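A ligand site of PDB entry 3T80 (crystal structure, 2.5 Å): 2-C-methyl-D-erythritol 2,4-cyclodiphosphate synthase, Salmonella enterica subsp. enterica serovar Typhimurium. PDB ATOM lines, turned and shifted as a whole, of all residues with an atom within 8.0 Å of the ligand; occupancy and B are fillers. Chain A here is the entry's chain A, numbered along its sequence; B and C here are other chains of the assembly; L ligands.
The guanidinium group (NH2) of Arg 145 of chain C is in salt-bridge range of an oxygen (O7) of the ligand, at 2.7 Å. N of Phe 142 of chain B is in hydrogen-bond range of O4 of the ligand (3.3 Å). NH2 of Arg 145 of chain B lies within salt-bridge range of O5 of the ligand. The backbone NH (N) of Phe 142 of chain A sits at hydrogen-bond distance from an oxygen (O3) of the ligand (2.9 Å). The backbone NH (N) of Phe 142 of chain C lies within hydrogen-bond range of an oxygen (O2) of the ligand. An oxygen (O5) of the ligand lies within salt-bridge range of the guanidinium group of Arg 145 of chain A, at 2.8 Å.
NH1 of Arg 145 of chain C sits close to O of Gly 141 of chain C (3.4 Å). The guanidinium group (NE) of Arg 145 of chain B lies within salt-bridge range of the side-chain carboxylate (OE2) of Glu 147 of chain B, at 2.8 Å. The backbone carbonyl oxygen (O) of Gly 141 of chain B lies close to the guanidinium group (NH1) of Arg 145 of chain B, 3.5 Å away. The backbone carbonyl oxygen (O) of Gly 141 of chain A sits close to the guanidinium group (NH1) of Arg 145 of chain A (3.4 Å). The backbone carbonyl oxygen (O) of Phe 142 of chain A sits at hydrogen-bond distance from the backbone NH (N) of Glu 147 of chain A (2.9 Å). The side-chain carboxylate (OE2) of Glu 147 of chain A lies within salt-bridge range of the guanidinium group (NE) of Arg 145 of chain A (2.7 Å). N of Glu 147 of chain B sits at hydrogen-bond distance from O of Phe 142 of chain B (2.8 Å).
Residues that only touch the ligand: Gly 141 of chain A (3.3 Å), Gly 141 of chain B (3.3 Å) and Gly 141 of chain C (3.2 Å). Hydrophobic or aromatic side chains within 4 Å of the ligand: Phe 142 of chain A, Phe 142 of chain B and Phe 142 of chain C. Within 4 Å of the ligand: Gly 141 of chain A, Phe 142 of chain A, Arg 145 of chain A, Gly 141 of chain B, Phe 142 of chain B, Arg 145 of chain B, Gly 141 of chain C, Phe 142 of chain C and Arg 145 of chain C. The nearest printed residue that does not touch the ligand is Thr 143 of chain C (4.9 Å).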
ATOM      1  N   THR A 137     -12.228 -24.844   9.473  1.00  0.00           N
ATOM      2  CA  THR A 137     -13.226 -24.364  10.456  1.00  0.00           C
ATOM      3  C   THR A 137     -14.565 -23.974   9.823  1.00  0.00           C
ATOM      4  O   THR A 137     -15.353 -23.241  10.376  1.00  0.00           O
ATOM      5  CB  THR A 137     -12.729 -23.162  11.273  1.00  0.00           C
ATOM      6  OG1 THR A 137     -12.508 -22.053  10.395  1.00  0.00           O
ATOM      7  CG2 THR A 137     -11.434 -23.533  12.036  1.00  0.00           C
ATOM      8  N   LYS A 139     -15.306 -22.030   7.347  1.00  0.00           N
ATOM      9  CA  LYS A 139     -15.471 -20.569   7.117  1.00  0.00           C
ATOM     10  C   LYS A 139     -15.804 -19.753   8.377  1.00  0.00           C
ATOM     11  O   LYS A 139     -16.252 -18.616   8.321  1.00  0.00           O
ATOM     12  CB  LYS A 139     -16.568 -20.338   6.084  1.00  0.00           C
ATOM     13  CG  LYS A 139     -16.069 -20.519   4.647  1.00  0.00           C
ATOM     14  CD  LYS A 139     -17.081 -21.301   3.829  1.00  0.00           C
ATOM     15  CE  LYS A 139     -16.899 -21.129   2.326  1.00  0.00           C
ATOM     16  NZ  LYS A 139     -18.164 -21.433   1.580  1.00  0.00           N
ATOM     17  N   LEU A 140     -15.575 -20.387   9.508  1.00  0.00           N
ATOM     18  CA  LEU A 140     -15.768 -19.725  10.814  1.00  0.00           C
ATOM     19  C   LEU A 140     -14.456 -19.208  11.351  1.00  0.00           C
ATOM     20  O   LEU A 140     -13.394 -19.797  11.177  1.00  0.00           O
ATOM     21  CB  LEU A 140     -16.391 -20.636  11.868  1.00  0.00           C
ATOM     22  CG  LEU A 140     -17.850 -21.037  11.642  1.00  0.00           C
ATOM     23  CD1 LEU A 140     -18.158 -22.193  12.568  1.00  0.00           C
ATOM     24  CD2 LEU A 140     -18.838 -19.906  11.843  1.00  0.00           C
ATOM     25  N   GLY A 141     -14.573 -18.108  12.041  1.00  0.00           N
ATOM     26  CA  GLY A 141     -13.439 -17.443  12.662  1.00  0.00           C
ATOM     27  C   GLY A 141     -12.370 -16.969  11.698  1.00  0.00           C
ATOM     28  O   GLY A 141     -12.564 -16.866  10.489  1.00  0.00           O
ATOM     29  N   PHE A 142     -11.204 -16.734  12.265  1.00  0.00           N
ATOM     30  CA  PHE A 142     -10.073 -16.091  11.539  1.00  0.00           C
ATOM     31  C   PHE A 142      -9.449 -17.003  10.480  1.00  0.00           C
ATOM     32  O   PHE A 142      -9.034 -16.558   9.407  1.00  0.00           O
ATOM     33  CB  PHE A 142      -9.015 -15.460  12.480  1.00  0.00           C
ATOM     34  CG  PHE A 142      -8.035 -16.427  13.079  1.00  0.00           C
ATOM     35  CD1 PHE A 142      -8.147 -16.822  14.386  1.00  0.00           C
ATOM     36  CD2 PHE A 142      -6.970 -16.871  12.340  1.00  0.00           C
ATOM     37  CE1 PHE A 142      -7.230 -17.688  14.948  1.00  0.00           C
ATOM     38  CE2 PHE A 142      -6.046 -17.739  12.880  1.00  0.00           C
ATOM     39  CZ  PHE A 142      -6.175 -18.156  14.191  1.00  0.00           C
ATOM     40  N   THR A 143      -9.344 -18.285  10.784  1.00  0.00           N
ATOM     41  CA  THR A 143      -8.896 -19.285   9.764  1.00  0.00           C
ATOM     42  C   THR A 143      -9.954 -19.378   8.634  1.00  0.00           C
ATOM     43  O   THR A 143      -9.674 -19.406   7.441  1.00  0.00           O
ATOM     44  CB  THR A 143      -8.562 -20.671  10.340  1.00  0.00           C
ATOM     45  OG1 THR A 143      -9.703 -21.250  10.978  1.00  0.00           O
ATOM     46  CG2 THR A 143      -7.395 -20.568  11.332  1.00  0.00           C
ATOM     47  N   GLY A 144     -11.192 -19.343   9.069  1.00  0.00           N
ATOM     48  CA  GLY A 144     -12.371 -19.490   8.167  1.00  0.00           C
ATOM     49  C   GLY A 144     -12.492 -18.407   7.105  1.00  0.00           C
ATOM     50  O   GLY A 144     -12.735 -18.658   5.933  1.00  0.00           O
ATOM     51  N   ARG A 145     -12.270 -17.201   7.571  1.00  0.00           N
ATOM     52  CA  ARG A 145     -12.203 -15.967   6.724  1.00  0.00           C
ATOM     53  C   ARG A 145     -10.902 -15.891   5.888  1.00  0.00           C
ATOM     54  O   ARG A 145     -10.656 -14.944   5.144  1.00  0.00           O
ATOM     55  CB  ARG A 145     -12.316 -14.705   7.577  1.00  0.00           C
ATOM     56  CG  ARG A 145     -13.657 -14.496   8.275  1.00  0.00           C
ATOM     57  CD  ARG A 145     -13.722 -13.114   8.924  1.00  0.00           C
ATOM     58  NE  ARG A 145     -12.762 -12.958  10.005  1.00  0.00           N
ATOM     59  CZ  ARG A 145     -12.959 -13.380  11.250  1.00  0.00           C
ATOM     60  NH1 ARG A 145     -14.093 -13.976  11.585  1.00  0.00           N
ATOM     61  NH2 ARG A 145     -11.997 -13.225  12.172  1.00  0.00           N
ATOM     62  N   GLU A 147      -7.811 -15.510   7.002  1.00  0.00           N
ATOM     63  CA  GLU A 147      -6.921 -14.452   7.547  1.00  0.00           C
ATOM     64  C   GLU A 147      -5.555 -15.019   7.947  1.00  0.00           C
ATOM     65  O   GLU A 147      -4.546 -14.330   8.029  1.00  0.00           O
ATOM     66  CB  GLU A 147      -7.572 -13.727   8.716  1.00  0.00           C
ATOM     67  CG  GLU A 147      -8.742 -12.879   8.255  1.00  0.00           C
ATOM     68  CD  GLU A 147      -9.598 -12.303   9.364  1.00  0.00           C
ATOM     69  OE1 GLU A 147      -9.284 -12.481  10.561  1.00  0.00           O
ATOM     70  OE2 GLU A 147     -10.616 -11.652   9.014  1.00  0.00           O
ATOM     71  N   THR B 137     -16.685 -19.846  25.540  1.00  0.00           N
ATOM     72  CA  THR B 137     -15.634 -18.863  25.251  1.00  0.00           C
ATOM     73  C   THR B 137     -16.051 -17.471  25.709  1.00  0.00           C
ATOM     74  O   THR B 137     -15.508 -16.466  25.286  1.00  0.00           O
ATOM     75  CB  THR B 137     -15.276 -18.831  23.779  1.00  0.00           C
ATOM     76  OG1 THR B 137     -16.466 -18.613  23.011  1.00  0.00           O
ATOM     77  CG2 THR B 137     -14.618 -20.127  23.399  1.00  0.00           C
ATOM     78  N   LYS B 139     -18.609 -15.634  25.282  1.00  0.00           N
ATOM     79  CA  LYS B 139     -19.205 -14.726  24.301  1.00  0.00           C
ATOM     80  C   LYS B 139     -18.169 -14.176  23.296  1.00  0.00           C
ATOM     81  O   LYS B 139     -18.447 -13.342  22.466  1.00  0.00           O
ATOM     82  CB  LYS B 139     -19.823 -13.556  25.064  1.00  0.00           C
ATOM     83  CG  LYS B 139     -21.260 -13.265  24.715  1.00  0.00           C
ATOM     84  CD  LYS B 139     -22.182 -14.354  25.223  1.00  0.00           C
ATOM     85  CE  LYS B 139     -23.646 -13.890  25.216  1.00  0.00           C
ATOM     86  NZ  LYS B 139     -24.467 -14.516  24.135  1.00  0.00           N
ATOM     87  N   LEU B 140     -16.954 -14.656  23.432  1.00  0.00           N
ATOM     88  CA  LEU B 140     -15.883 -14.375  22.449  1.00  0.00           C
ATOM     89  C   LEU B 140     -15.756 -15.374  21.319  1.00  0.00           C
ATOM     90  O   LEU B 140     -16.102 -16.545  21.431  1.00  0.00           O
ATOM     91  CB  LEU B 140     -14.525 -14.255  23.093  1.00  0.00           C
ATOM     92  CG  LEU B 140     -14.477 -13.216  24.180  1.00  0.00           C
ATOM     93  CD1 LEU B 140     -13.088 -13.257  24.813  1.00  0.00           C
ATOM     94  CD2 LEU B 140     -14.844 -11.830  23.654  1.00  0.00           C
ATOM     95  N   GLY B 141     -15.153 -14.868  20.256  1.00  0.00           N
ATOM     96  CA  GLY B 141     -15.054 -15.559  18.933  1.00  0.00           C
ATOM     97  C   GLY B 141     -16.329 -16.142  18.321  1.00  0.00           C
ATOM     98  O   GLY B 141     -17.436 -15.863  18.745  1.00  0.00           O
ATOM     99  N   PHE B 142     -16.139 -16.964  17.298  1.00  0.00           N
ATOM    100  CA  PHE B 142     -17.274 -17.542  16.520  1.00  0.00           C
ATOM    101  C   PHE B 142     -18.217 -18.406  17.381  1.00  0.00           C
ATOM    102  O   PHE B 142     -19.442 -18.405  17.195  1.00  0.00           O
ATOM    103  CB  PHE B 142     -16.850 -18.263  15.230  1.00  0.00           C
ATOM    104  CG  PHE B 142     -16.137 -19.563  15.424  1.00  0.00           C
ATOM    105  CD1 PHE B 142     -14.747 -19.611  15.385  1.00  0.00           C
ATOM    106  CD2 PHE B 142     -16.836 -20.744  15.554  1.00  0.00           C
ATOM    107  CE1 PHE B 142     -14.085 -20.806  15.525  1.00  0.00           C
ATOM    108  CE2 PHE B 142     -16.185 -21.937  15.704  1.00  0.00           C
ATOM    109  CZ  PHE B 142     -14.804 -21.971  15.695  1.00  0.00           C
ATOM    110  N   THR B 143     -17.635 -19.123  18.325  1.00  0.00           N
ATOM    111  CA  THR B 143     -18.432 -19.903  19.319  1.00  0.00           C
ATOM    112  C   THR B 143     -19.276 -18.934  20.180  1.00  0.00           C
ATOM    113  O   THR B 143     -20.508 -19.009  20.302  1.00  0.00           O
ATOM    114  CB  THR B 143     -17.591 -20.866  20.212  1.00  0.00           C
ATOM    115  OG1 THR B 143     -16.504 -20.179  20.841  1.00  0.00           O
ATOM    116  CG2 THR B 143     -17.066 -22.035  19.352  1.00  0.00           C
ATOM    117  N   GLY B 144     -18.556 -17.958  20.684  1.00  0.00           N
ATOM    118  CA  GLY B 144     -19.095 -16.865  21.529  1.00  0.00           C
ATOM    119  C   GLY B 144     -20.257 -16.079  20.946  1.00  0.00           C
ATOM    120  O   GLY B 144     -21.185 -15.667  21.631  1.00  0.00           O
ATOM    121  N   ARG B 145     -20.172 -15.913  19.636  1.00  0.00           N
ATOM    122  CA  ARG B 145     -21.201 -15.154  18.842  1.00  0.00           C
ATOM    123  C   ARG B 145     -22.351 -16.058  18.439  1.00  0.00           C
ATOM    124  O   ARG B 145     -23.329 -15.655  17.829  1.00  0.00           O
ATOM    125  CB  ARG B 145     -20.604 -14.486  17.605  1.00  0.00           C
ATOM    126  CG  ARG B 145     -19.680 -13.290  17.927  1.00  0.00           C
ATOM    127  CD  ARG B 145     -19.315 -12.463  16.698  1.00  0.00           C
ATOM    128  NE  ARG B 145     -18.637 -13.277  15.695  1.00  0.00           N
ATOM    129  CZ  ARG B 145     -17.345 -13.603  15.721  1.00  0.00           C
ATOM    130  NH1 ARG B 145     -16.546 -13.186  16.703  1.00  0.00           N
ATOM    131  NH2 ARG B 145     -16.842 -14.366  14.756  1.00  0.00           N
ATOM    132  N   GLU B 147     -22.105 -18.628  16.429  1.00  0.00           N
ATOM    133  CA  GLU B 147     -21.987 -18.873  14.955  1.00  0.00           C
ATOM    134  C   GLU B 147     -21.801 -20.332  14.676  1.00  0.00           C
ATOM    135  O   GLU B 147     -22.079 -20.839  13.604  1.00  0.00           O
ATOM    136  CB  GLU B 147     -20.849 -18.071  14.341  1.00  0.00           C
ATOM    137  CG  GLU B 147     -21.284 -16.633  14.042  1.00  0.00           C
ATOM    138  CD  GLU B 147     -20.133 -15.691  13.778  1.00  0.00           C
ATOM    139  OE1 GLU B 147     -19.015 -16.165  13.572  1.00  0.00           O
ATOM    140  OE2 GLU B 147     -20.373 -14.450  13.791  1.00  0.00           O
ATOM    141  N   THR C 137      -1.513 -14.905  18.862  1.00  0.00           N
ATOM    142  CA  THR C 137      -2.188 -15.301  17.595  1.00  0.00           C
ATOM    143  C   THR C 137      -2.012 -14.277  16.464  1.00  0.00           C
ATOM    144  O   THR C 137      -2.772 -14.220  15.491  1.00  0.00           O
ATOM    145  CB  THR C 137      -3.665 -15.543  17.767  1.00  0.00           C
ATOM    146  OG1 THR C 137      -4.266 -14.333  18.228  1.00  0.00           O
ATOM    147  CG2 THR C 137      -3.900 -16.668  18.728  1.00  0.00           C
ATOM    148  N   LYS C 139      -2.256 -10.977  16.268  1.00  0.00           N
ATOM    149  CA  LYS C 139      -3.350  -9.978  16.065  1.00  0.00           C
ATOM    150  C   LYS C 139      -4.641 -10.565  15.455  1.00  0.00           C
ATOM    151  O   LYS C 139      -5.589  -9.849  15.110  1.00  0.00           O
ATOM    152  CB  LYS C 139      -2.885  -8.802  15.186  1.00  0.00           C
ATOM    153  CG  LYS C 139      -1.985  -7.792  15.891  1.00  0.00           C
ATOM    154  CD  LYS C 139      -2.758  -6.951  16.911  1.00  0.00           C
ATOM    155  CE  LYS C 139      -1.943  -5.807  17.518  1.00  0.00           C
ATOM    156  NZ  LYS C 139      -2.601  -5.251  18.740  1.00  0.00           N
ATOM    157  N   LEU C 140      -4.635 -11.884  15.305  1.00  0.00           N
ATOM    158  CA  LEU C 140      -5.798 -12.611  14.758  1.00  0.00           C
ATOM    159  C   LEU C 140      -6.738 -13.106  15.821  1.00  0.00           C
ATOM    160  O   LEU C 140      -6.358 -13.571  16.891  1.00  0.00           O
ATOM    161  CB  LEU C 140      -5.420 -13.805  13.863  1.00  0.00           C
ATOM    162  CG  LEU C 140      -4.544 -13.495  12.650  1.00  0.00           C
ATOM    163  CD1 LEU C 140      -4.367 -14.724  11.768  1.00  0.00           C
ATOM    164  CD2 LEU C 140      -5.112 -12.327  11.851  1.00  0.00           C
ATOM    165  N   GLY C 141      -8.004 -12.990  15.491  1.00  0.00           N
ATOM    166  CA  GLY C 141      -9.092 -13.508  16.311  1.00  0.00           C
ATOM    167  C   GLY C 141      -9.357 -12.688  17.550  1.00  0.00           C
ATOM    168  O   GLY C 141      -8.815 -11.599  17.722  1.00  0.00           O
ATOM    169  N   PHE C 142     -10.189 -13.211  18.428  1.00  0.00           N
ATOM    170  CA  PHE C 142     -10.551 -12.458  19.675  1.00  0.00           C
ATOM    171  C   PHE C 142      -9.343 -12.252  20.611  1.00  0.00           C
ATOM    172  O   PHE C 142      -9.251 -11.251  21.309  1.00  0.00           O
ATOM    173  CB  PHE C 142     -11.736 -13.047  20.438  1.00  0.00           C
ATOM    174  CG  PHE C 142     -11.458 -14.358  21.100  1.00  0.00           C
ATOM    175  CD1 PHE C 142     -10.961 -14.400  22.376  1.00  0.00           C
ATOM    176  CD2 PHE C 142     -11.736 -15.534  20.434  1.00  0.00           C
ATOM    177  CE1 PHE C 142     -10.719 -15.607  22.988  1.00  0.00           C
ATOM    178  CE2 PHE C 142     -11.509 -16.757  21.043  1.00  0.00           C
ATOM    179  CZ  PHE C 142     -10.989 -16.789  22.321  1.00  0.00           C
ATOM    180  N   THR C 143      -8.446 -13.202  20.634  1.00  0.00           N
ATOM    181  CA  THR C 143      -7.190 -13.010  21.431  1.00  0.00           C
ATOM    182  C   THR C 143      -6.366 -11.880  20.824  1.00  0.00           C
ATOM    183  O   THR C 143      -5.861 -10.979  21.482  1.00  0.00           O
ATOM    184  CB  THR C 143      -6.321 -14.266  21.527  1.00  0.00           C
ATOM    185  OG1 THR C 143      -6.293 -14.941  20.260  1.00  0.00           O
ATOM    186  CG2 THR C 143      -6.905 -15.197  22.595  1.00  0.00           C
ATOM    187  N   GLY C 144      -6.314 -11.951  19.504  1.00  0.00           N
ATOM    188  CA  GLY C 144      -5.511 -11.050  18.662  1.00  0.00           C
ATOM    189  C   GLY C 144      -5.913  -9.589  18.723  1.00  0.00           C
ATOM    190  O   GLY C 144      -5.094  -8.710  18.737  1.00  0.00           O
ATOM    191  N   ARG C 145      -7.218  -9.380  18.757  1.00  0.00           N
ATOM    192  CA  ARG C 145      -7.855  -8.033  18.892  1.00  0.00           C
ATOM    193  C   ARG C 145      -7.927  -7.529  20.321  1.00  0.00           C
ATOM    194  O   ARG C 145      -8.567  -6.507  20.627  1.00  0.00           O
ATOM    195  CB  ARG C 145      -9.274  -8.030  18.361  1.00  0.00           C
ATOM    196  CG  ARG C 145      -9.399  -8.387  16.897  1.00  0.00           C
ATOM    197  CD  ARG C 145     -10.841  -8.300  16.446  1.00  0.00           C
ATOM    198  NE  ARG C 145     -11.731  -9.176  17.196  1.00  0.00           N
ATOM    199  CZ  ARG C 145     -12.027 -10.426  16.848  1.00  0.00           C
ATOM    200  NH1 ARG C 145     -11.500 -10.959  15.786  1.00  0.00           N
ATOM    201  NH2 ARG C 145     -12.855 -11.139  17.598  1.00  0.00           N
ATOM    202  N   GLU C 147      -9.362  -8.904  22.937  1.00  0.00           N
ATOM    203  CA  GLU C 147     -10.722  -9.055  23.544  1.00  0.00           C
ATOM    204  C   GLU C 147     -10.707  -9.992  24.741  1.00  0.00           C
ATOM    205  O   GLU C 147     -11.559  -9.960  25.642  1.00  0.00           O
ATOM    206  CB  GLU C 147     -11.720  -9.574  22.534  1.00  0.00           C
ATOM    207  CG  GLU C 147     -12.205  -8.474  21.614  1.00  0.00           C
ATOM    208  CD  GLU C 147     -12.830  -8.996  20.352  1.00  0.00           C
ATOM    209  OE1 GLU C 147     -13.065 -10.215  20.242  1.00  0.00           O
ATOM    210  OE2 GLU C 147     -13.073  -8.170  19.443  1.00  0.00           O
HETATM  211  P1  LIG L   1     -11.883 -16.662  16.478  1.00  0.00           P
HETATM  212  O1  LIG L   1     -12.334 -17.869  17.269  1.00  0.00           O
HETATM  213  O2  LIG L   1     -10.961 -15.835  17.326  1.00  0.00           O
HETATM  214  O3  LIG L   1     -11.247 -17.089  15.165  1.00  0.00           O
HETATM  215  O4  LIG L   1     -13.234 -15.860  16.141  1.00  0.00           O
HETATM  216  P2  LIG L   1     -13.281 -14.405  15.484  1.00  0.00           P
HETATM  217  O5  LIG L   1     -14.245 -14.495  14.343  1.00  0.00           O
HETATM  218  O6  LIG L   1     -11.969 -13.904  15.012  1.00  0.00           O
HETATM  219  O7  LIG L   1     -13.790 -13.522  16.594  1.00  0.00           O
